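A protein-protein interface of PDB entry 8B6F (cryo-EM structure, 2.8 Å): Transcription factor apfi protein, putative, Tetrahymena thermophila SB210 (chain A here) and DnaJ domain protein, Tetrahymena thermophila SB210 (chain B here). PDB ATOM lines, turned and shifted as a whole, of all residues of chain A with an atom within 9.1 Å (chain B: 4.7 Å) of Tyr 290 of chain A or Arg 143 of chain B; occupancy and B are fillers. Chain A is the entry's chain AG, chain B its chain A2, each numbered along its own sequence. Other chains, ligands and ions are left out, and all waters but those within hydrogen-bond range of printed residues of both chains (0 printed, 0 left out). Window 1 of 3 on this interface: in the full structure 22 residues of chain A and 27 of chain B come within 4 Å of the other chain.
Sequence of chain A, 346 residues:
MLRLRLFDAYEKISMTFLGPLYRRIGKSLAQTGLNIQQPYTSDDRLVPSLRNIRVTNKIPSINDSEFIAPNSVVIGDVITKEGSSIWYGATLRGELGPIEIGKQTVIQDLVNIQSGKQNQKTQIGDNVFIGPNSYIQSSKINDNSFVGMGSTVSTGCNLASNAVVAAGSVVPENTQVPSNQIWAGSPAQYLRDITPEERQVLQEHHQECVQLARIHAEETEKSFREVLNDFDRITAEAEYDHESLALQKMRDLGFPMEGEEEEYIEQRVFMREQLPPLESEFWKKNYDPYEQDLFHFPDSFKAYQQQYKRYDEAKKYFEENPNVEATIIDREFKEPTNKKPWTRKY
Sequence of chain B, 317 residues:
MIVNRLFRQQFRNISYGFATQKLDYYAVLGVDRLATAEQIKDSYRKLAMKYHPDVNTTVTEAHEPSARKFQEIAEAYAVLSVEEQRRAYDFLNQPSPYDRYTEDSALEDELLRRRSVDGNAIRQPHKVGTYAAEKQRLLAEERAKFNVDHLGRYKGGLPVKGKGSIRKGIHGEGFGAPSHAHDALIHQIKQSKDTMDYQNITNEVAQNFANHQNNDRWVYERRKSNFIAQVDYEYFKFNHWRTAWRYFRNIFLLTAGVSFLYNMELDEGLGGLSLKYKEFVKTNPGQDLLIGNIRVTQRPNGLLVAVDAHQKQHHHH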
ATOM      1  N   ASN A 286      18.726   6.436 -21.665  1.00  0.00           N
ATOM      2  CA  ASN A 286      17.612   5.904 -20.897  1.00  0.00           C
ATOM      3  C   ASN A 286      16.391   6.790 -21.089  1.00  0.00           C
ATOM      4  O   ASN A 286      16.503   8.010 -21.223  1.00  0.00           O
ATOM      5  CB  ASN A 286      17.962   5.810 -19.409  1.00  0.00           C
ATOM      6  CG  ASN A 286      16.957   5.001 -18.626  1.00  0.00           C
ATOM      7  OD1 ASN A 286      16.199   4.215 -19.193  1.00  0.00           O
ATOM      8  ND2 ASN A 286      16.946   5.184 -17.314  1.00  0.00           N
ATOM      9  N   TYR A 287      15.214   6.159 -21.086  1.00  0.00           N
ATOM     10  CA  TYR A 287      13.947   6.860 -21.263  1.00  0.00           C
ATOM     11  C   TYR A 287      13.011   6.665 -20.077  1.00  0.00           C
ATOM     12  O   TYR A 287      11.809   6.919 -20.194  1.00  0.00           O
ATOM     13  CB  TYR A 287      13.260   6.402 -22.550  1.00  0.00           C
ATOM     14  CG  TYR A 287      13.998   6.795 -23.807  1.00  0.00           C
ATOM     15  CD1 TYR A 287      13.853   8.065 -24.351  1.00  0.00           C
ATOM     16  CD2 TYR A 287      14.836   5.897 -24.452  1.00  0.00           C
ATOM     17  CE1 TYR A 287      14.524   8.429 -25.498  1.00  0.00           C
ATOM     18  CE2 TYR A 287      15.512   6.251 -25.599  1.00  0.00           C
ATOM     19  CZ  TYR A 287      15.351   7.518 -26.117  1.00  0.00           C
ATOM     20  OH  TYR A 287      16.022   7.875 -27.262  1.00  0.00           O
ATOM     21  N   ASP A 288      13.531   6.218 -18.938  1.00  0.00           N
ATOM     22  CA  ASP A 288      12.691   6.049 -17.767  1.00  0.00           C
ATOM     23  C   ASP A 288      12.169   7.405 -17.295  1.00  0.00           C
ATOM     24  O   ASP A 288      12.865   8.418 -17.405  1.00  0.00           O
ATOM     25  CB  ASP A 288      13.468   5.375 -16.640  1.00  0.00           C
ATOM     26  CG  ASP A 288      13.814   3.936 -16.951  1.00  0.00           C
ATOM     27  OD1 ASP A 288      13.441   3.458 -18.042  1.00  0.00           O
ATOM     28  OD2 ASP A 288      14.458   3.281 -16.106  1.00  0.00           O
ATOM     29  N   PRO A 289      10.946   7.455 -16.772  1.00  0.00           N
ATOM     30  CA  PRO A 289      10.420   8.734 -16.283  1.00  0.00           C
ATOM     31  C   PRO A 289      11.291   9.290 -15.169  1.00  0.00           C
ATOM     32  O   PRO A 289      11.796   8.552 -14.321  1.00  0.00           O
ATOM     33  CB  PRO A 289       9.013   8.379 -15.787  1.00  0.00           C
ATOM     34  CG  PRO A 289       9.047   6.914 -15.545  1.00  0.00           C
ATOM     35  CD  PRO A 289       9.997   6.350 -16.550  1.00  0.00           C
ATOM     36  N   TYR A 290      11.469  10.607 -15.182  1.00  0.00           N
ATOM     37  CA  TYR A 290      12.329  11.251 -14.203  1.00  0.00           C
ATOM     38  C   TYR A 290      11.710  11.191 -12.814  1.00  0.00           C
ATOM     39  O   TYR A 290      10.501  11.366 -12.644  1.00  0.00           O
ATOM     40  CB  TYR A 290      12.582  12.704 -14.593  1.00  0.00           C
ATOM     41  CG  TYR A 290      13.319  13.486 -13.536  1.00  0.00           C
ATOM     42  CD1 TYR A 290      14.702  13.432 -13.443  1.00  0.00           C
ATOM     43  CD2 TYR A 290      12.631  14.277 -12.628  1.00  0.00           C
ATOM     44  CE1 TYR A 290      15.379  14.146 -12.476  1.00  0.00           C
ATOM     45  CE2 TYR A 290      13.297  14.993 -11.659  1.00  0.00           C
ATOM     46  CZ  TYR A 290      14.671  14.924 -11.587  1.00  0.00           C
ATOM     47  OH  TYR A 290      15.336  15.637 -10.620  1.00  0.00           O
ATOM     48  N   GLU A 291      12.553  10.940 -11.817  1.00  0.00           N
ATOM     49  CA  GLU A 291      12.145  10.970 -10.423  1.00  0.00           C
ATOM     50  C   GLU A 291      13.288  11.531  -9.594  1.00  0.00           C
ATOM     51  O   GLU A 291      14.459  11.385  -9.948  1.00  0.00           O
ATOM     52  CB  GLU A 291      11.755   9.578  -9.917  1.00  0.00           C
ATOM     53  CG  GLU A 291      12.842   8.537 -10.100  1.00  0.00           C
ATOM     54  CD  GLU A 291      12.389   7.153  -9.695  1.00  0.00           C
ATOM     55  OE1 GLU A 291      11.246   7.020  -9.210  1.00  0.00           O
ATOM     56  OE2 GLU A 291      13.174   6.197  -9.862  1.00  0.00           O
ATOM     57  N   GLN A 292      12.937  12.179  -8.488  1.00  0.00           N
ATOM     58  CA  GLN A 292      13.946  12.784  -7.633  1.00  0.00           C
ATOM     59  C   GLN A 292      14.865  11.707  -7.072  1.00  0.00           C
ATOM     60  O   GLN A 292      14.404  10.669  -6.587  1.00  0.00           O
ATOM     61  CB  GLN A 292      13.276  13.563  -6.499  1.00  0.00           C
ATOM     62  CG  GLN A 292      14.089  14.742  -5.987  1.00  0.00           C
ATOM     63  CD  GLN A 292      15.343  14.317  -5.259  1.00  0.00           C
ATOM     64  OE1 GLN A 292      15.278  13.628  -4.243  1.00  0.00           O
ATOM     65  NE2 GLN A 292      16.496  14.721  -5.780  1.00  0.00           N
ATOM     66  N   ASP A 293      16.170  11.953  -7.142  1.00  0.00           N
ATOM     67  CA  ASP A 293      17.146  11.006  -6.620  1.00  0.00           C
ATOM     68  C   ASP A 293      17.090  11.005  -5.099  1.00  0.00           C
ATOM     69  O   ASP A 293      17.408  12.012  -4.459  1.00  0.00           O
ATOM     70  CB  ASP A 293      18.545  11.373  -7.106  1.00  0.00           C
ATOM     71  CG  ASP A 293      19.585  10.343  -6.723  1.00  0.00           C
ATOM     72  OD1 ASP A 293      19.202   9.277  -6.198  1.00  0.00           O
ATOM     73  OD2 ASP A 293      20.785  10.598  -6.944  1.00  0.00           O
ATOM     74  N   LEU A 294      16.691   9.875  -4.519  1.00  0.00           N
ATOM     75  CA  LEU A 294      16.477   9.769  -3.084  1.00  0.00           C
ATOM     76  C   LEU A 294      17.742   9.393  -2.324  1.00  0.00           C
ATOM     77  O   LEU A 294      17.653   8.833  -1.227  1.00  0.00           O
ATOM     78  CB  LEU A 294      15.358   8.770  -2.792  1.00  0.00           C
ATOM     79  CG  LEU A 294      14.001   9.125  -3.410  1.00  0.00           C
ATOM     80  CD1 LEU A 294      12.947   8.136  -2.970  1.00  0.00           C
ATOM     81  CD2 LEU A 294      13.565  10.542  -3.063  1.00  0.00           C
ATOM     82  N   PHE A 295      18.911   9.668  -2.892  1.00  0.00           N
ATOM     83  CA  PHE A 295      20.148   9.599  -2.130  1.00  0.00           C
ATOM     84  C   PHE A 295      20.143  10.695  -1.069  1.00  0.00           C
ATOM     85  O   PHE A 295      19.711  11.822  -1.324  1.00  0.00           O
ATOM     86  CB  PHE A 295      21.348   9.762  -3.064  1.00  0.00           C
ATOM     87  CG  PHE A 295      22.585   9.050  -2.600  1.00  0.00           C
ATOM     88  CD1 PHE A 295      22.709   7.679  -2.754  1.00  0.00           C
ATOM     89  CD2 PHE A 295      23.636   9.755  -2.038  1.00  0.00           C
ATOM     90  CE1 PHE A 295      23.851   7.021  -2.340  1.00  0.00           C
ATOM     91  CE2 PHE A 295      24.781   9.104  -1.623  1.00  0.00           C
ATOM     92  CZ  PHE A 295      24.889   7.735  -1.775  1.00  0.00           C
ATOM     93  N   HIS A 296      20.628  10.362   0.123  1.00  0.00           N
ATOM     94  CA  HIS A 296      20.645  11.211   1.311  1.00  0.00           C
ATOM     95  C   HIS A 296      19.292  11.248   2.015  1.00  0.00           C
ATOM     96  O   HIS A 296      19.185  11.885   3.067  1.00  0.00           O
ATOM     97  CB  HIS A 296      21.053  12.664   1.012  1.00  0.00           C
ATOM     98  CG  HIS A 296      22.315  12.793   0.219  1.00  0.00           C
ATOM     99  ND1 HIS A 296      23.533  12.340   0.678  1.00  0.00           N
ATOM    100  CD2 HIS A 296      22.551  13.339  -0.996  1.00  0.00           C
ATOM    101  CE1 HIS A 296      24.463  12.596  -0.223  1.00  0.00           C
ATOM    102  NE2 HIS A 296      23.895  13.203  -1.249  1.00  0.00           N
ATOM    103  N   PHE A 297      18.268  10.596   1.487  1.00  0.00           N
ATOM    104  CA  PHE A 297      16.951  10.579   2.104  1.00  0.00           C
ATOM    105  C   PHE A 297      16.805   9.359   2.999  1.00  0.00           C
ATOM    106  O   PHE A 297      17.601   8.420   2.937  1.00  0.00           O
ATOM    107  CB  PHE A 297      15.876  10.594   1.021  1.00  0.00           C
ATOM    108  CG  PHE A 297      15.730  11.919   0.332  1.00  0.00           C
ATOM    109  CD1 PHE A 297      16.684  12.357  -0.571  1.00  0.00           C
ATOM    110  CD2 PHE A 297      14.631  12.722   0.578  1.00  0.00           C
ATOM    111  CE1 PHE A 297      16.546  13.573  -1.210  1.00  0.00           C
ATOM    112  CE2 PHE A 297      14.488  13.938  -0.055  1.00  0.00           C
ATOM    113  CZ  PHE A 297      15.448  14.364  -0.952  1.00  0.00           C
ATOM    114  N   GLN A 305      11.969   4.590  -4.371  1.00  0.00           N
ATOM    115  CA  GLN A 305      12.850   4.733  -5.517  1.00  0.00           C
ATOM    116  C   GLN A 305      12.714   3.522  -6.439  1.00  0.00           C
ATOM    117  O   GLN A 305      12.321   2.429  -6.022  1.00  0.00           O
ATOM    118  CB  GLN A 305      14.299   4.886  -5.050  1.00  0.00           C
ATOM    119  CG  GLN A 305      15.316   5.116  -6.161  1.00  0.00           C
ATOM    120  CD  GLN A 305      15.120   6.436  -6.876  1.00  0.00           C
ATOM    121  OE1 GLN A 305      15.023   6.484  -8.101  1.00  0.00           O
ATOM    122  NE2 GLN A 305      15.082   7.520  -6.115  1.00  0.00           N
ATOM    123  N   GLN A 306      13.037   3.732  -7.711  1.00  0.00           N
ATOM    124  CA  GLN A 306      13.023   2.637  -8.670  1.00  0.00           C
ATOM    125  C   GLN A 306      13.950   1.521  -8.202  1.00  0.00           C
ATOM    126  O   GLN A 306      15.052   1.771  -7.706  1.00  0.00           O
ATOM    127  CB  GLN A 306      13.444   3.139 -10.050  1.00  0.00           C
ATOM    128  CG  GLN A 306      13.474   2.065 -11.127  1.00  0.00           C
ATOM    129  CD  GLN A 306      13.871   2.615 -12.483  1.00  0.00           C
ATOM    130  OE1 GLN A 306      14.741   2.066 -13.156  1.00  0.00           O
ATOM    131  NE2 GLN A 306      13.226   3.700 -12.894  1.00  0.00           N
ATOM    132  N   LEU B 139      20.338  10.917 -13.704  1.00  0.00           N
ATOM    133  CA  LEU B 139      19.516  11.893 -12.998  1.00  0.00           C
ATOM    134  C   LEU B 139      20.297  13.167 -12.715  1.00  0.00           C
ATOM    135  O   LEU B 139      19.736  14.268 -12.758  1.00  0.00           O
ATOM    136  CB  LEU B 139      18.976  11.291 -11.703  1.00  0.00           C
ATOM    137  CG  LEU B 139      17.980  10.139 -11.861  1.00  0.00           C
ATOM    138  CD1 LEU B 139      17.599   9.573 -10.503  1.00  0.00           C
ATOM    139  CD2 LEU B 139      16.739  10.590 -12.615  1.00  0.00           C
ATOM    140  N   ALA B 140      21.593  13.045 -12.429  1.00  0.00           N
ATOM    141  CA  ALA B 140      22.418  14.237 -12.272  1.00  0.00           C
ATOM    142  C   ALA B 140      22.438  15.052 -13.557  1.00  0.00           C
ATOM    143  O   ALA B 140      22.338  16.283 -13.523  1.00  0.00           O
ATOM    144  CB  ALA B 140      23.837  13.843 -11.863  1.00  0.00           C
ATOM    145  N   GLU B 141      22.569  14.381 -14.703  1.00  0.00           N
ATOM    146  CA  GLU B 141      22.539  15.086 -15.979  1.00  0.00           C
ATOM    147  C   GLU B 141      21.192  15.764 -16.198  1.00  0.00           C
ATOM    148  O   GLU B 141      21.132  16.897 -16.689  1.00  0.00           O
ATOM    149  CB  GLU B 141      22.845  14.118 -17.121  1.00  0.00           C
ATOM    150  CG  GLU B 141      24.268  13.583 -17.104  1.00  0.00           C
ATOM    151  CD  GLU B 141      24.534  12.606 -18.232  1.00  0.00           C
ATOM    152  OE1 GLU B 141      23.635  12.414 -19.076  1.00  0.00           O
ATOM    153  OE2 GLU B 141      25.642  12.028 -18.274  1.00  0.00           O
ATOM    154  N   GLU B 142      20.098  15.083 -15.850  1.00  0.00           N
ATOM    155  CA  GLU B 142      18.773  15.678 -16.009  1.00  0.00           C
ATOM    156  C   GLU B 142      18.625  16.925 -15.147  1.00  0.00           C
ATOM    157  O   GLU B 142      18.119  17.956 -15.605  1.00  0.00           O
ATOM    158  CB  GLU B 142      17.693  14.657 -15.648  1.00  0.00           C
ATOM    159  CG  GLU B 142      17.642  13.448 -16.563  1.00  0.00           C
ATOM    160  CD  GLU B 142      17.108  13.778 -17.941  1.00  0.00           C
ATOM    161  OE1 GLU B 142      16.619  14.910 -18.137  1.00  0.00           O
ATOM    162  OE2 GLU B 142      17.179  12.904 -18.829  1.00  0.00           O
ATOM    163  N   ARG B 143      19.061  16.850 -13.888  1.00  0.00           N
ATOM    164  CA  ARG B 143      18.972  18.009 -13.006  1.00  0.00           C
ATOM    165  C   ARG B 143      19.831  19.156 -13.515  1.00  0.00           C
ATOM    166  O   ARG B 143      19.431  20.324 -13.441  1.00  0.00           O
ATOM    167  CB  ARG B 143      19.379  17.621 -11.585  1.00  0.00           C
ATOM    168  CG  ARG B 143      18.397  16.691 -10.896  1.00  0.00           C
ATOM    169  CD  ARG B 143      18.654  16.631  -9.401  1.00  0.00           C
ATOM    170  NE  ARG B 143      20.044  16.304  -9.102  1.00  0.00           N
ATOM    171  CZ  ARG B 143      20.515  15.072  -8.965  1.00  0.00           C
ATOM    172  NH1 ARG B 143      19.733  14.012  -9.091  1.00  0.00           N
ATOM    173  NH2 ARG B 143      21.805  14.898  -8.693  1.00  0.00           N
ATOM    174  N   ALA B 144      21.015  18.846 -14.042  1.00  0.00           N
ATOM    175  CA  ALA B 144      21.851  19.882 -14.637  1.00  0.00           C
ATOM    176  C   ALA B 144      21.149  20.541 -15.816  1.00  0.00           C
ATOM    177  O   ALA B 144      21.204  21.765 -15.976  1.00  0.00           O
ATOM    178  CB  ALA B 144      23.190  19.289 -15.075  1.00  0.00           C
ATOM    179  N   LYS B 145      20.481  19.746 -16.653  1.00  0.00           N
ATOM    180  CA  LYS B 145      19.765  20.315 -17.789  1.00  0.00           C
ATOM    181  C   LYS B 145      18.665  21.264 -17.332  1.00  0.00           C
ATOM    182  O   LYS B 145      18.467  22.327 -17.929  1.00  0.00           O
ATOM    183  CB  LYS B 145      19.180  19.194 -18.651  1.00  0.00           C
ATOM    184  CG  LYS B 145      20.221  18.418 -19.448  1.00  0.00           C
ATOM    185  CD  LYS B 145      19.570  17.336 -20.301  1.00  0.00           C
ATOM    186  CE  LYS B 145      20.605  16.556 -21.099  1.00  0.00           C
ATOM    187  NZ  LYS B 145      21.359  17.424 -22.046  1.00  0.00           N
ATOM    188  N   PHE B 146      17.933  20.898 -16.284  1.00  0.00           N
ATOM    189  CA  PHE B 146      16.811  21.698 -15.811  1.00  0.00           C
ATOM    190  C   PHE B 146      17.200  22.715 -14.743  1.00  0.00           C
ATOM    191  O   PHE B 146      16.317  23.389 -14.206  1.00  0.00           O
ATOM    192  CB  PHE B 146      15.708  20.785 -15.271  1.00  0.00           C
ATOM    193  CG  PHE B 146      14.590  20.562 -16.242  1.00  0.00           C
ATOM    194  CD1 PHE B 146      14.649  19.523 -17.154  1.00  0.00           C
ATOM    195  CD2 PHE B 146      13.492  21.401 -16.259  1.00  0.00           C
ATOM    196  CE1 PHE B 146      13.628  19.315 -18.055  1.00  0.00           C
ATOM    197  CE2 PHE B 146      12.466  21.199 -17.159  1.00  0.00           C
ATOM    198  CZ  PHE B 146      12.535  20.155 -18.058  1.00  0.00           C
ATOM    199  N   ASN B 147      18.486  22.846 -14.422  1.00  0.00           N
ATOM    200  CA  ASN B 147      18.957  23.825 -13.444  1.00  0.00           C
ATOM    201  C   ASN B 147      18.378  23.544 -12.055  1.00  0.00           C
ATOM    202  O   ASN B 147      17.735  24.390 -11.435  1.00  0.00           O
ATOM    203  CB  ASN B 147      18.621  25.247 -13.902  1.00  0.00           C
ATOM    204  CG  ASN B 147      19.231  26.305 -13.008  1.00  0.00           C
ATOM    205  OD1 ASN B 147      20.288  26.101 -12.417  1.00  0.00           O
ATOM    206  ND2 ASN B 147      18.563  27.445 -12.902  1.00  0.00           N
ATOM    207  N   VAL B 148      18.625  22.327 -11.573  1.00  0.00           N
ATOM    208  CA  VAL B 148      18.144  21.874 -10.274  1.00  0.00           C
ATOM    209  C   VAL B 148      19.324  21.331  -9.482  1.00  0.00           C
ATOM    210  O   VAL B 148      20.169  20.614 -10.025  1.00  0.00           O
ATOM    211  CB  VAL B 148      17.045  20.800 -10.424  1.00  0.00           C
ATOM    212  CG1 VAL B 148      16.571  20.317  -9.063  1.00  0.00           C
ATOM    213  CG2 VAL B 148      15.886  21.349 -11.226  1.00  0.00           C
ATOM    214  N   ASP B 149      19.386  21.682  -8.200  1.00  0.00           N
ATOM    215  CA  ASP B 149      20.486  21.257  -7.349  1.00  0.00           C
ATOM    216  C   ASP B 149      20.305  19.794  -6.949  1.00  0.00           C
ATOM    217  O   ASP B 149      19.317  19.143  -7.293  1.00  0.00           O
ATOM    218  CB  ASP B 149      20.594  22.161  -6.122  1.00  0.00           C
ATOM    219  CG  ASP B 149      19.391  22.057  -5.205  1.00  0.00           C
ATOM    220  OD1 ASP B 149      18.445  21.313  -5.534  1.00  0.00           O
ATOM    221  OD2 ASP B 149      19.390  22.727  -4.150  1.00  0.00           O
ATOM    222  N   HIS B 150      21.278  19.268  -6.203  1.00  0.00           N
ATOM    223  CA  HIS B 150      21.273  17.851  -5.861  1.00  0.00           C
ATOM    224  C   HIS B 150      20.101  17.465  -4.966  1.00  0.00           C
ATOM    225  O   HIS B 150      19.747  16.283  -4.915  1.00  0.00           O
ATOM    226  CB  HIS B 150      22.591  17.472  -5.183  1.00  0.00           C
ATOM    227  CG  HIS B 150      22.840  18.192  -3.895  1.00  0.00           C
ATOM    228  ND1 HIS B 150      23.270  19.501  -3.843  1.00  0.00           N
ATOM    229  CD2 HIS B 150      22.727  17.783  -2.610  1.00  0.00           C
ATOM    230  CE1 HIS B 150      23.405  19.868  -2.582  1.00  0.00           C
ATOM    231  NE2 HIS B 150      23.083  18.844  -1.813  1.00  0.00           N
ATOM    232  N   HIS B 182      11.712  21.428  -7.611  1.00  0.00           N
ATOM    233  CA  HIS B 182      11.491  20.924  -8.956  1.00  0.00           C
ATOM    234  C   HIS B 182      10.319  19.951  -8.972  1.00  0.00           C
ATOM    235  O   HIS B 182      10.108  19.194  -8.023  1.00  0.00           O
ATOM    236  CB  HIS B 182      12.755  20.239  -9.469  1.00  0.00           C
ATOM    237  CG  HIS B 182      12.680  19.833 -10.904  1.00  0.00           C
ATOM    238  ND1 HIS B 182      12.184  20.662 -11.887  1.00  0.00           N
ATOM    239  CD2 HIS B 182      13.045  18.689 -11.526  1.00  0.00           C
ATOM    240  CE1 HIS B 182      12.244  20.044 -13.052  1.00  0.00           C
ATOM    241  NE2 HIS B 182      12.763  18.844 -12.859  1.00  0.00           N
ATOM    242  N   ALA B 184       8.515  16.790 -10.718  1.00  0.00           N
ATOM    243  CA  ALA B 184       8.778  15.635 -11.571  1.00  0.00           C
ATOM    244  C   ALA B 184       7.776  15.542 -12.714  1.00  0.00           C
ATOM    245  O   ALA B 184       8.142  15.190 -13.841  1.00  0.00           O
ATOM    246  CB  ALA B 184       8.755  14.355 -10.736  1.00  0.00           C
ATOM    247  N   HIS B 187       8.740  18.032 -15.302  1.00  0.00           N
ATOM    248  CA  HIS B 187       9.916  17.527 -16.001  1.00  0.00           C
ATOM    249  C   HIS B 187       9.526  16.475 -17.030  1.00  0.00           C
ATOM    250  O   HIS B 187      10.016  16.493 -18.165  1.00  0.00           O
ATOM    251  CB  HIS B 187      10.914  16.950 -14.997  1.00  0.00           C
ATOM    252  CG  HIS B 187      12.184  16.455 -15.620  1.00  0.00           C
ATOM    253  ND1 HIS B 187      13.383  17.122 -15.502  1.00  0.00           N
ATOM    254  CD2 HIS B 187      12.440  15.353 -16.362  1.00  0.00           C
ATOM    255  CE1 HIS B 187      14.322  16.454 -16.146  1.00  0.00           C
ATOM    256  NE2 HIS B 187      13.776  15.376 -16.677  1.00  0.00           N
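The side-chain carboxylate (OE2) of Glu 291 of chain A lies close to the side-chain amide oxygen (OE1) of Gln 305 of chain A.
The side-chain carboxylate (OE2) of Glu 291 of chain A sits close to the backbone NH (N) of Gln 306 of chain A (3.3 Å).
NE2 of Gln 305 of chain A is in hydrogen-bond range of O of Gln 292 of chain A, 3.3 Å away.
N of Phe 295 of chain A lies close to OD1 of Asp 293 of chain A.
The backbone carbonyl oxygen (O) of Arg 143 of chain B sits at hydrogen-bond distance from the backbone NH (N) of Val 148 of chain B (2.9 Å).
A ring nitrogen (ND1) of His 187 of chain B sits at hydrogen-bond distance from a ring nitrogen (NE2) of His 182 of chain B, 3.2 Å away.
Of the 14 printed residues of chain A, 4 touch a printed residue of chain B.
Printed residues of chain A that touch a printed residue of chain B: Tyr 290, Glu 291, Gln 292 and Asp 293.
Along chain A the printed residues that touch a printed residue of chain B span positions 290 to 293.
Printed residues of chain B that touch a printed residue of chain A: Leu 139, Glu 142, Arg 143, His 150, His 182, Ala 184 and His 187.
Among the printed residues, 10 pairs touch across the chains.
Among the printed residues, no Asp or Glu carboxylate lies within 4 Å of a Lys or Arg side-chain nitrogen of the other chain.
CD1 of Tyr 290 of chain A touches CD2 of Leu 139 of chain B, 3.6 Å away.
Tyr 290 of chain A touches Glu 142 of chain B (CD1 to CB, 3.9 Å).
Arg 143 of chain B touches Tyr 290 of chain A (CG to OH, 3.2 Å).
Tyr 290 of chain A touches His 182 of chain B.
CB of Ala 184 of chain B touches O of Tyr 290 of chain A (3.95 Å).
CB of Tyr 290 of chain A touches CD2 of His 187 of chain B, 3.2 Å away.
Glu 291 of chain A touches Leu 139 of chain B (O to CD2, 3.6 Å).
O of His 150 of chain B touches NE2 of Gln 292 of chain A (3.7 Å).
Leu 139 of chain B touches Asp 293 of chain A (CD1 to CB, 3.96 Å).
NH1 of Arg 143 of chain B touches CB of Asp 293 of chain A, at 3.5 Å.
Of chain B, only Leu 139, Glu 142, Arg 143, His 182, Ala 184 and His 187 come within 4 Å of Tyr 290 of chain A.
Of the printed residues of chain B, Asp 293 of chain A touches Leu 139 and Arg 143.
Of chain A, only Tyr 290 (3.2 Å) and Asp 293 (3.5 Å) come within 4 Å of Arg 143 of chain B.
No residue of chain A comes within 4 Å of Ala 144 of chain B.
No residue of chain A comes within 4 Å of Val 148 of chain B.
Of the printed residues of chain A, His 150 of chain B touches Gln 292 (3.7 Å).
The nearest printed residue of chain B that does not touch Tyr 290 of chain A is Val 148 of chain B (5.1 Å).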
